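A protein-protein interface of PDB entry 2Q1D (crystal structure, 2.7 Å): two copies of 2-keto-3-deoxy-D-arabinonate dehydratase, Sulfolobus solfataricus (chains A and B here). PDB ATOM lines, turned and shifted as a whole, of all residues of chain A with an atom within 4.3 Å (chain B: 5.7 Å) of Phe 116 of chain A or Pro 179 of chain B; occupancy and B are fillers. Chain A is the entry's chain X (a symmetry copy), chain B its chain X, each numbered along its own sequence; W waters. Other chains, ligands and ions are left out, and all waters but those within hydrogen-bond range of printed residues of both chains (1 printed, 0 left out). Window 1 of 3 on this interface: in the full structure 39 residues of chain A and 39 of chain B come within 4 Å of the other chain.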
ATOM      1  N   TRP A  77      28.736  24.152  36.306  1.00  0.00           N
ATOM      2  CA  TRP A  77      28.575  24.497  34.892  1.00  0.00           C
ATOM      3  C   TRP A  77      29.672  23.809  34.100  1.00  0.00           C
ATOM      4  O   TRP A  77      30.811  23.660  34.586  1.00  0.00           O
ATOM      5  CB  TRP A  77      28.706  26.015  34.666  1.00  0.00           C
ATOM      6  CG  TRP A  77      27.536  26.816  35.160  1.00  0.00           C
ATOM      7  CD1 TRP A  77      27.288  27.197  36.447  1.00  0.00           C
ATOM      8  CD2 TRP A  77      26.462  27.337  34.374  1.00  0.00           C
ATOM      9  NE1 TRP A  77      26.121  27.916  36.513  1.00  0.00           N
ATOM     10  CE2 TRP A  77      25.594  28.016  35.252  1.00  0.00           C
ATOM     11  CE3 TRP A  77      26.145  27.290  33.014  1.00  0.00           C
ATOM     12  CZ2 TRP A  77      24.432  28.637  34.817  1.00  0.00           C
ATOM     13  CZ3 TRP A  77      24.995  27.912  32.584  1.00  0.00           C
ATOM     14  CH2 TRP A  77      24.152  28.575  33.483  1.00  0.00           C
ATOM     15  N   GLY A  78      29.343  23.446  32.862  1.00  0.00           N
ATOM     16  CA  GLY A  78      30.303  22.812  31.974  1.00  0.00           C
ATOM     17  C   GLY A  78      30.646  23.582  30.717  1.00  0.00           C
ATOM     18  O   GLY A  78      29.825  24.332  30.174  1.00  0.00           O
ATOM     19  N   SER A  79      31.874  23.375  30.256  1.00  0.00           N
ATOM     20  CA  SER A  79      32.328  23.861  28.962  1.00  0.00           C
ATOM     21  C   SER A  79      32.440  22.698  27.965  1.00  0.00           C
ATOM     22  O   SER A  79      32.762  21.558  28.343  1.00  0.00           O
ATOM     23  CB  SER A  79      33.685  24.538  29.111  1.00  0.00           C
ATOM     24  OG  SER A  79      33.718  25.771  28.416  1.00  0.00           O
ATOM     25  N   GLU A 114      30.989  26.923  23.886  1.00  0.00           N
ATOM     26  CA  GLU A 114      29.839  26.253  24.492  1.00  0.00           C
ATOM     27  C   GLU A 114      29.932  26.312  26.016  1.00  0.00           C
ATOM     28  O   GLU A 114      31.010  26.088  26.601  1.00  0.00           O
ATOM     29  CB  GLU A 114      29.733  24.795  24.042  1.00  0.00           C
ATOM     30  CG  GLU A 114      28.459  24.084  24.552  1.00  0.00           C
ATOM     31  CD  GLU A 114      28.441  22.577  24.297  1.00  0.00           C
ATOM     32  OE1 GLU A 114      29.436  22.036  23.759  1.00  0.00           O
ATOM     33  OE2 GLU A 114      27.416  21.932  24.637  1.00  0.00           O
ATOM     34  N   ILE A 115      28.796  26.628  26.640  1.00  0.00           N
ATOM     35  CA  ILE A 115      28.657  26.636  28.087  1.00  0.00           C
ATOM     36  C   ILE A 115      27.305  26.007  28.409  1.00  0.00           C
ATOM     37  O   ILE A 115      26.283  26.381  27.808  1.00  0.00           O
ATOM     38  CB  ILE A 115      28.718  28.075  28.654  1.00  0.00           C
ATOM     39  CG1 ILE A 115      30.089  28.711  28.417  1.00  0.00           C
ATOM     40  CG2 ILE A 115      28.385  28.096  30.144  1.00  0.00           C
ATOM     41  CD1 ILE A 115      31.149  28.321  29.412  1.00  0.00           C
ATOM     42  N   PHE A 116      27.290  25.041  29.331  1.00  0.00           N
ATOM     43  CA  PHE A 116      26.029  24.415  29.737  1.00  0.00           C
ATOM     44  C   PHE A 116      25.926  24.276  31.247  1.00  0.00           C
ATOM     45  O   PHE A 116      26.941  24.217  31.954  1.00  0.00           O
ATOM     46  CB  PHE A 116      25.825  23.044  29.049  1.00  0.00           C
ATOM     47  CG  PHE A 116      26.880  22.019  29.407  1.00  0.00           C
ATOM     48  CD1 PHE A 116      26.689  21.154  30.475  1.00  0.00           C
ATOM     49  CD2 PHE A 116      28.079  21.943  28.684  1.00  0.00           C
ATOM     50  CE1 PHE A 116      27.679  20.224  30.806  1.00  0.00           C
ATOM     51  CE2 PHE A 116      29.068  21.027  29.006  1.00  0.00           C
ATOM     52  CZ  PHE A 116      28.874  20.163  30.065  1.00  0.00           C
ATOM     53  N   PHE A 117      24.695  24.220  31.740  1.00  0.00           N
ATOM     54  CA  PHE A 117      24.468  23.930  33.141  1.00  0.00           C
ATOM     55  C   PHE A 117      24.695  22.430  33.372  1.00  0.00           C
ATOM     56  O   PHE A 117      24.080  21.596  32.683  1.00  0.00           O
ATOM     57  CB  PHE A 117      23.053  24.329  33.552  1.00  0.00           C
ATOM     58  CG  PHE A 117      22.819  24.279  35.024  1.00  0.00           C
ATOM     59  CD1 PHE A 117      22.066  23.245  35.591  1.00  0.00           C
ATOM     60  CD2 PHE A 117      23.353  25.244  35.856  1.00  0.00           C
ATOM     61  CE1 PHE A 117      21.833  23.179  36.983  1.00  0.00           C
ATOM     62  CE2 PHE A 117      23.135  25.193  37.236  1.00  0.00           C
ATOM     63  CZ  PHE A 117      22.367  24.151  37.801  1.00  0.00           C
ATOM     64  N   LYS A 118      25.563  22.098  34.334  1.00  0.00           N
ATOM     65  CA  LYS A 118      25.883  20.700  34.653  1.00  0.00           C
ATOM     66  C   LYS A 118      25.098  20.092  35.824  1.00  0.00           C
ATOM     67  O   LYS A 118      24.421  19.071  35.637  1.00  0.00           O
ATOM     68  CB  LYS A 118      27.394  20.496  34.854  1.00  0.00           C
ATOM     69  CG  LYS A 118      27.803  19.045  35.172  1.00  0.00           C
ATOM     70  CD  LYS A 118      27.222  18.007  34.193  1.00  0.00           C
ATOM     71  CE  LYS A 118      27.552  16.591  34.648  1.00  0.00           C
ATOM     72  NZ  LYS A 118      26.865  15.510  33.864  1.00  0.00           N
ATOM     73  N   ASP A 164      32.450  14.742  34.356  1.00  0.00           N
ATOM     74  CA  ASP A 164      31.250  15.138  33.644  1.00  0.00           C
ATOM     75  C   ASP A 164      30.593  13.901  33.009  1.00  0.00           C
ATOM     76  O   ASP A 164      30.654  13.688  31.806  1.00  0.00           O
ATOM     77  CB  ASP A 164      31.633  16.194  32.597  1.00  0.00           C
ATOM     78  CG  ASP A 164      30.469  16.615  31.695  1.00  0.00           C
ATOM     79  OD1 ASP A 164      29.268  16.490  32.066  1.00  0.00           O
ATOM     80  OD2 ASP A 164      30.779  17.095  30.578  1.00  0.00           O
ATOM     81  N   LYS A 182      22.944  15.296  30.466  1.00  0.00           N
ATOM     82  CA  LYS A 182      23.970  15.854  31.365  1.00  0.00           C
ATOM     83  C   LYS A 182      23.586  15.987  32.853  1.00  0.00           C
ATOM     84  O   LYS A 182      24.465  15.954  33.720  1.00  0.00           O
ATOM     85  CB  LYS A 182      24.465  17.210  30.836  1.00  0.00           C
ATOM     86  CG  LYS A 182      25.326  17.145  29.568  1.00  0.00           C
ATOM     87  CD  LYS A 182      26.757  16.737  29.874  1.00  0.00           C
ATOM     88  CE  LYS A 182      27.596  16.828  28.639  1.00  0.00           C
ATOM     89  NZ  LYS A 182      29.014  16.542  28.928  1.00  0.00           N
ATOM     90  N   PRO B 175      22.533  25.313  18.332  1.00  0.00           N
ATOM     91  CA  PRO B 175      21.774  24.795  19.488  1.00  0.00           C
ATOM     92  C   PRO B 175      22.628  24.535  20.746  1.00  0.00           C
ATOM     93  O   PRO B 175      22.086  24.485  21.850  1.00  0.00           O
ATOM     94  CB  PRO B 175      21.167  23.491  18.964  1.00  0.00           C
ATOM     95  CG  PRO B 175      22.060  23.085  17.810  1.00  0.00           C
ATOM     96  CD  PRO B 175      22.543  24.372  17.194  1.00  0.00           C
ATOM     97  N   LEU B 176      23.940  24.386  20.595  1.00  0.00           N
ATOM     98  CA  LEU B 176      24.808  24.222  21.757  1.00  0.00           C
ATOM     99  C   LEU B 176      24.896  25.493  22.604  1.00  0.00           C
ATOM    100  O   LEU B 176      25.506  25.498  23.684  1.00  0.00           O
ATOM    101  CB  LEU B 176      26.202  23.764  21.339  1.00  0.00           C
ATOM    102  CG  LEU B 176      26.225  22.392  20.680  1.00  0.00           C
ATOM    103  CD1 LEU B 176      27.587  22.106  20.082  1.00  0.00           C
ATOM    104  CD2 LEU B 176      25.815  21.306  21.683  1.00  0.00           C
ATOM    105  N   TYR B 177      24.287  26.565  22.109  1.00  0.00           N
ATOM    106  CA  TYR B 177      24.204  27.815  22.842  1.00  0.00           C
ATOM    107  C   TYR B 177      22.879  27.947  23.581  1.00  0.00           C
ATOM    108  O   TYR B 177      22.635  28.962  24.255  1.00  0.00           O
ATOM    109  CB  TYR B 177      24.374  29.002  21.902  1.00  0.00           C
ATOM    110  CG  TYR B 177      25.717  29.113  21.210  1.00  0.00           C
ATOM    111  CD1 TYR B 177      26.900  28.736  21.846  1.00  0.00           C
ATOM    112  CD2 TYR B 177      25.801  29.644  19.923  1.00  0.00           C
ATOM    113  CE1 TYR B 177      28.127  28.867  21.207  1.00  0.00           C
ATOM    114  CE2 TYR B 177      27.020  29.778  19.281  1.00  0.00           C
ATOM    115  CZ  TYR B 177      28.176  29.394  19.924  1.00  0.00           C
ATOM    116  OH  TYR B 177      29.378  29.535  19.266  1.00  0.00           O
ATOM    117  N   LEU B 178      22.029  26.924  23.479  1.00  0.00           N
ATOM    118  CA  LEU B 178      20.724  26.968  24.131  1.00  0.00           C
ATOM    119  C   LEU B 178      20.801  27.372  25.618  1.00  0.00           C
ATOM    120  O   LEU B 178      20.024  28.222  26.060  1.00  0.00           O
ATOM    121  CB  LEU B 178      19.959  25.658  23.952  1.00  0.00           C
ATOM    122  CG  LEU B 178      18.456  25.721  24.283  1.00  0.00           C
ATOM    123  CD1 LEU B 178      17.696  26.403  23.136  1.00  0.00           C
ATOM    124  CD2 LEU B 178      17.841  24.330  24.624  1.00  0.00           C
ATOM    125  N   PRO B 179      21.743  26.780  26.389  1.00  0.00           N
ATOM    126  CA  PRO B 179      21.853  27.185  27.787  1.00  0.00           C
ATOM    127  C   PRO B 179      22.117  28.686  27.959  1.00  0.00           C
ATOM    128  O   PRO B 179      21.406  29.348  28.722  1.00  0.00           O
ATOM    129  CB  PRO B 179      23.053  26.371  28.288  1.00  0.00           C
ATOM    130  CG  PRO B 179      23.101  25.211  27.400  1.00  0.00           C
ATOM    131  CD  PRO B 179      22.736  25.742  26.065  1.00  0.00           C
ATOM    132  N   GLN B 180      23.122  29.202  27.248  1.00  0.00           N
ATOM    133  CA  GLN B 180      23.472  30.624  27.299  1.00  0.00           C
ATOM    134  C   GLN B 180      22.266  31.452  26.889  1.00  0.00           C
ATOM    135  O   GLN B 180      22.024  32.524  27.440  1.00  0.00           O
ATOM    136  CB  GLN B 180      24.666  30.948  26.392  1.00  0.00           C
ATOM    137  CG  GLN B 180      25.989  30.308  26.823  1.00  0.00           C
ATOM    138  CD  GLN B 180      27.156  30.678  25.899  1.00  0.00           C
ATOM    139  OE1 GLN B 180      27.581  31.840  25.844  1.00  0.00           O
ATOM    140  NE2 GLN B 180      27.683  29.686  25.175  1.00  0.00           N
ATOM    141  N   SER B 181      21.489  30.923  25.950  1.00  0.00           N
ATOM    142  CA  SER B 181      20.316  31.614  25.457  1.00  0.00           C
ATOM    143  C   SER B 181      19.168  31.601  26.456  1.00  0.00           C
ATOM    144  O   SER B 181      18.295  32.456  26.387  1.00  0.00           O
ATOM    145  CB  SER B 181      19.853  30.994  24.142  1.00  0.00           C
ATOM    146  OG  SER B 181      18.742  30.142  24.342  1.00  0.00           O
ATOM    147  N   LYS B 182      19.176  30.643  27.384  1.00  0.00           N
ATOM    148  CA  LYS B 182      18.040  30.423  28.298  1.00  0.00           C
ATOM    149  C   LYS B 182      18.247  30.840  29.768  1.00  0.00           C
ATOM    150  O   LYS B 182      17.273  31.162  30.458  1.00  0.00           O
ATOM    151  CB  LYS B 182      17.581  28.956  28.236  1.00  0.00           C
ATOM    152  CG  LYS B 182      16.874  28.544  26.939  1.00  0.00           C
ATOM    153  CD  LYS B 182      15.427  29.004  26.910  1.00  0.00           C
ATOM    154  CE  LYS B 182      14.735  28.458  25.701  1.00  0.00           C
ATOM    155  NZ  LYS B 182      13.300  28.798  25.702  1.00  0.00           N
ATOM    156  N   ILE B 183      19.501  30.835  30.236  1.00  0.00           N
ATOM    157  CA  ILE B 183      19.821  30.948  31.673  1.00  0.00           C
ATOM    158  C   ILE B 183      20.685  32.156  31.934  1.00  0.00           C
ATOM    159  O   ILE B 183      21.843  32.153  31.554  1.00  0.00           O
ATOM    160  CB  ILE B 183      20.631  29.686  32.190  1.00  0.00           C
ATOM    161  CG1 ILE B 183      19.920  28.367  31.829  1.00  0.00           C
ATOM    162  CG2 ILE B 183      20.916  29.778  33.705  1.00  0.00           C
ATOM    163  CD1 ILE B 183      20.758  27.099  32.085  1.00  0.00           C
ATOM    164  N   TYR B 184      20.137  33.168  32.604  1.00  0.00           N
ATOM    165  CA  TYR B 184      20.888  34.396  32.969  1.00  0.00           C
ATOM    166  C   TYR B 184      19.997  35.266  33.881  1.00  0.00           C
ATOM    167  O   TYR B 184      18.781  35.042  33.969  1.00  0.00           O
ATOM    168  CB  TYR B 184      21.331  35.204  31.716  1.00  0.00           C
ATOM    169  CG  TYR B 184      20.169  35.545  30.810  1.00  0.00           C
ATOM    170  CD1 TYR B 184      19.426  36.703  31.015  1.00  0.00           C
ATOM    171  CD2 TYR B 184      19.783  34.692  29.783  1.00  0.00           C
ATOM    172  CE1 TYR B 184      18.333  37.020  30.208  1.00  0.00           C
ATOM    173  CE2 TYR B 184      18.690  34.991  28.967  1.00  0.00           C
ATOM    174  CZ  TYR B 184      17.963  36.164  29.187  1.00  0.00           C
ATOM    175  OH  TYR B 184      16.863  36.482  28.402  1.00  0.00           O
HETATM  176  O   HOH W   1      26.296  27.338  25.355  1.00  0.00           O
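O of Phe 116 of chain A lies within hydrogen-bond range of N of Gly 78 of chain A, 2.7 Å away.
The backbone carbonyl oxygen (O) of Glu 114 of chain A sits at hydrogen-bond distance from the side-chain hydroxyl (OG) of Ser 79 of chain A (3.3 Å).
Water W1 lies within hydrogen-bond range of the backbone carbonyl oxygen (O) of Leu 176 of chain B (2.6 Å), the backbone carbonyl oxygen (O) of Ile 115 of chain A (2.6 Å) and the side-chain amide nitrogen (NE2) of Gln 180 of chain B (2.7 Å).
Among the printed residues, pairs that only touch across the chains: Ile 115 of chain A with Pro 179 of chain B (3.3 Å), Glu 114 of chain A with Leu 176 of chain B (3.4 Å), Trp 77 of chain A with Ile 183 of chain B (3.5 Å), Ile 115 of chain A with Gln 180 of chain B (3.6 Å), Phe 116 of chain A with Pro 179 of chain B (3.8 Å) and Phe 117 of chain A with Ile 183 of chain B (3.9 Å).
Ser 79 of chain A touches none of the printed residues of chain B.
Of the printed residues of chain B, Glu 114 of chain A touches Leu 176.
Pro 179 of chain B touches two residues of chain A.
Printed residues of chain A within 4 Å of Ile 183 of chain B: Trp 77 and Phe 117.
The nearest printed residue of chain B that does not touch Phe 116 of chain A is Leu 176 of chain B (5.9 Å).
The nearest printed residue of chain A that does not touch Pro 179 of chain B is Phe 117 of chain A (4.4 Å).
Hydrophobic or aromatic side chains of chain A that line the printed part of chain B: Trp 77, Ile 115, Phe 116 and Phe 117.
Along chain A the printed residues that touch a printed residue of chain B span positions 77 to 117.
Printed residues of chain B that touch a printed residue of chain A: Leu 176, Pro 179, Gln 180 and Ile 183.
Hydrophobic or aromatic side chains of chain B within 4 Å of the printed part of chain A: Leu 176, Pro 179 and Ile 183.
Among the printed residues, 6 pairs touch across the chains.
Among the printed residues, no Asp or Glu carboxylate lies within 4 Å of a Lys or Arg side-chain nitrogen of the other chain.
1 position is printed for both chains.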
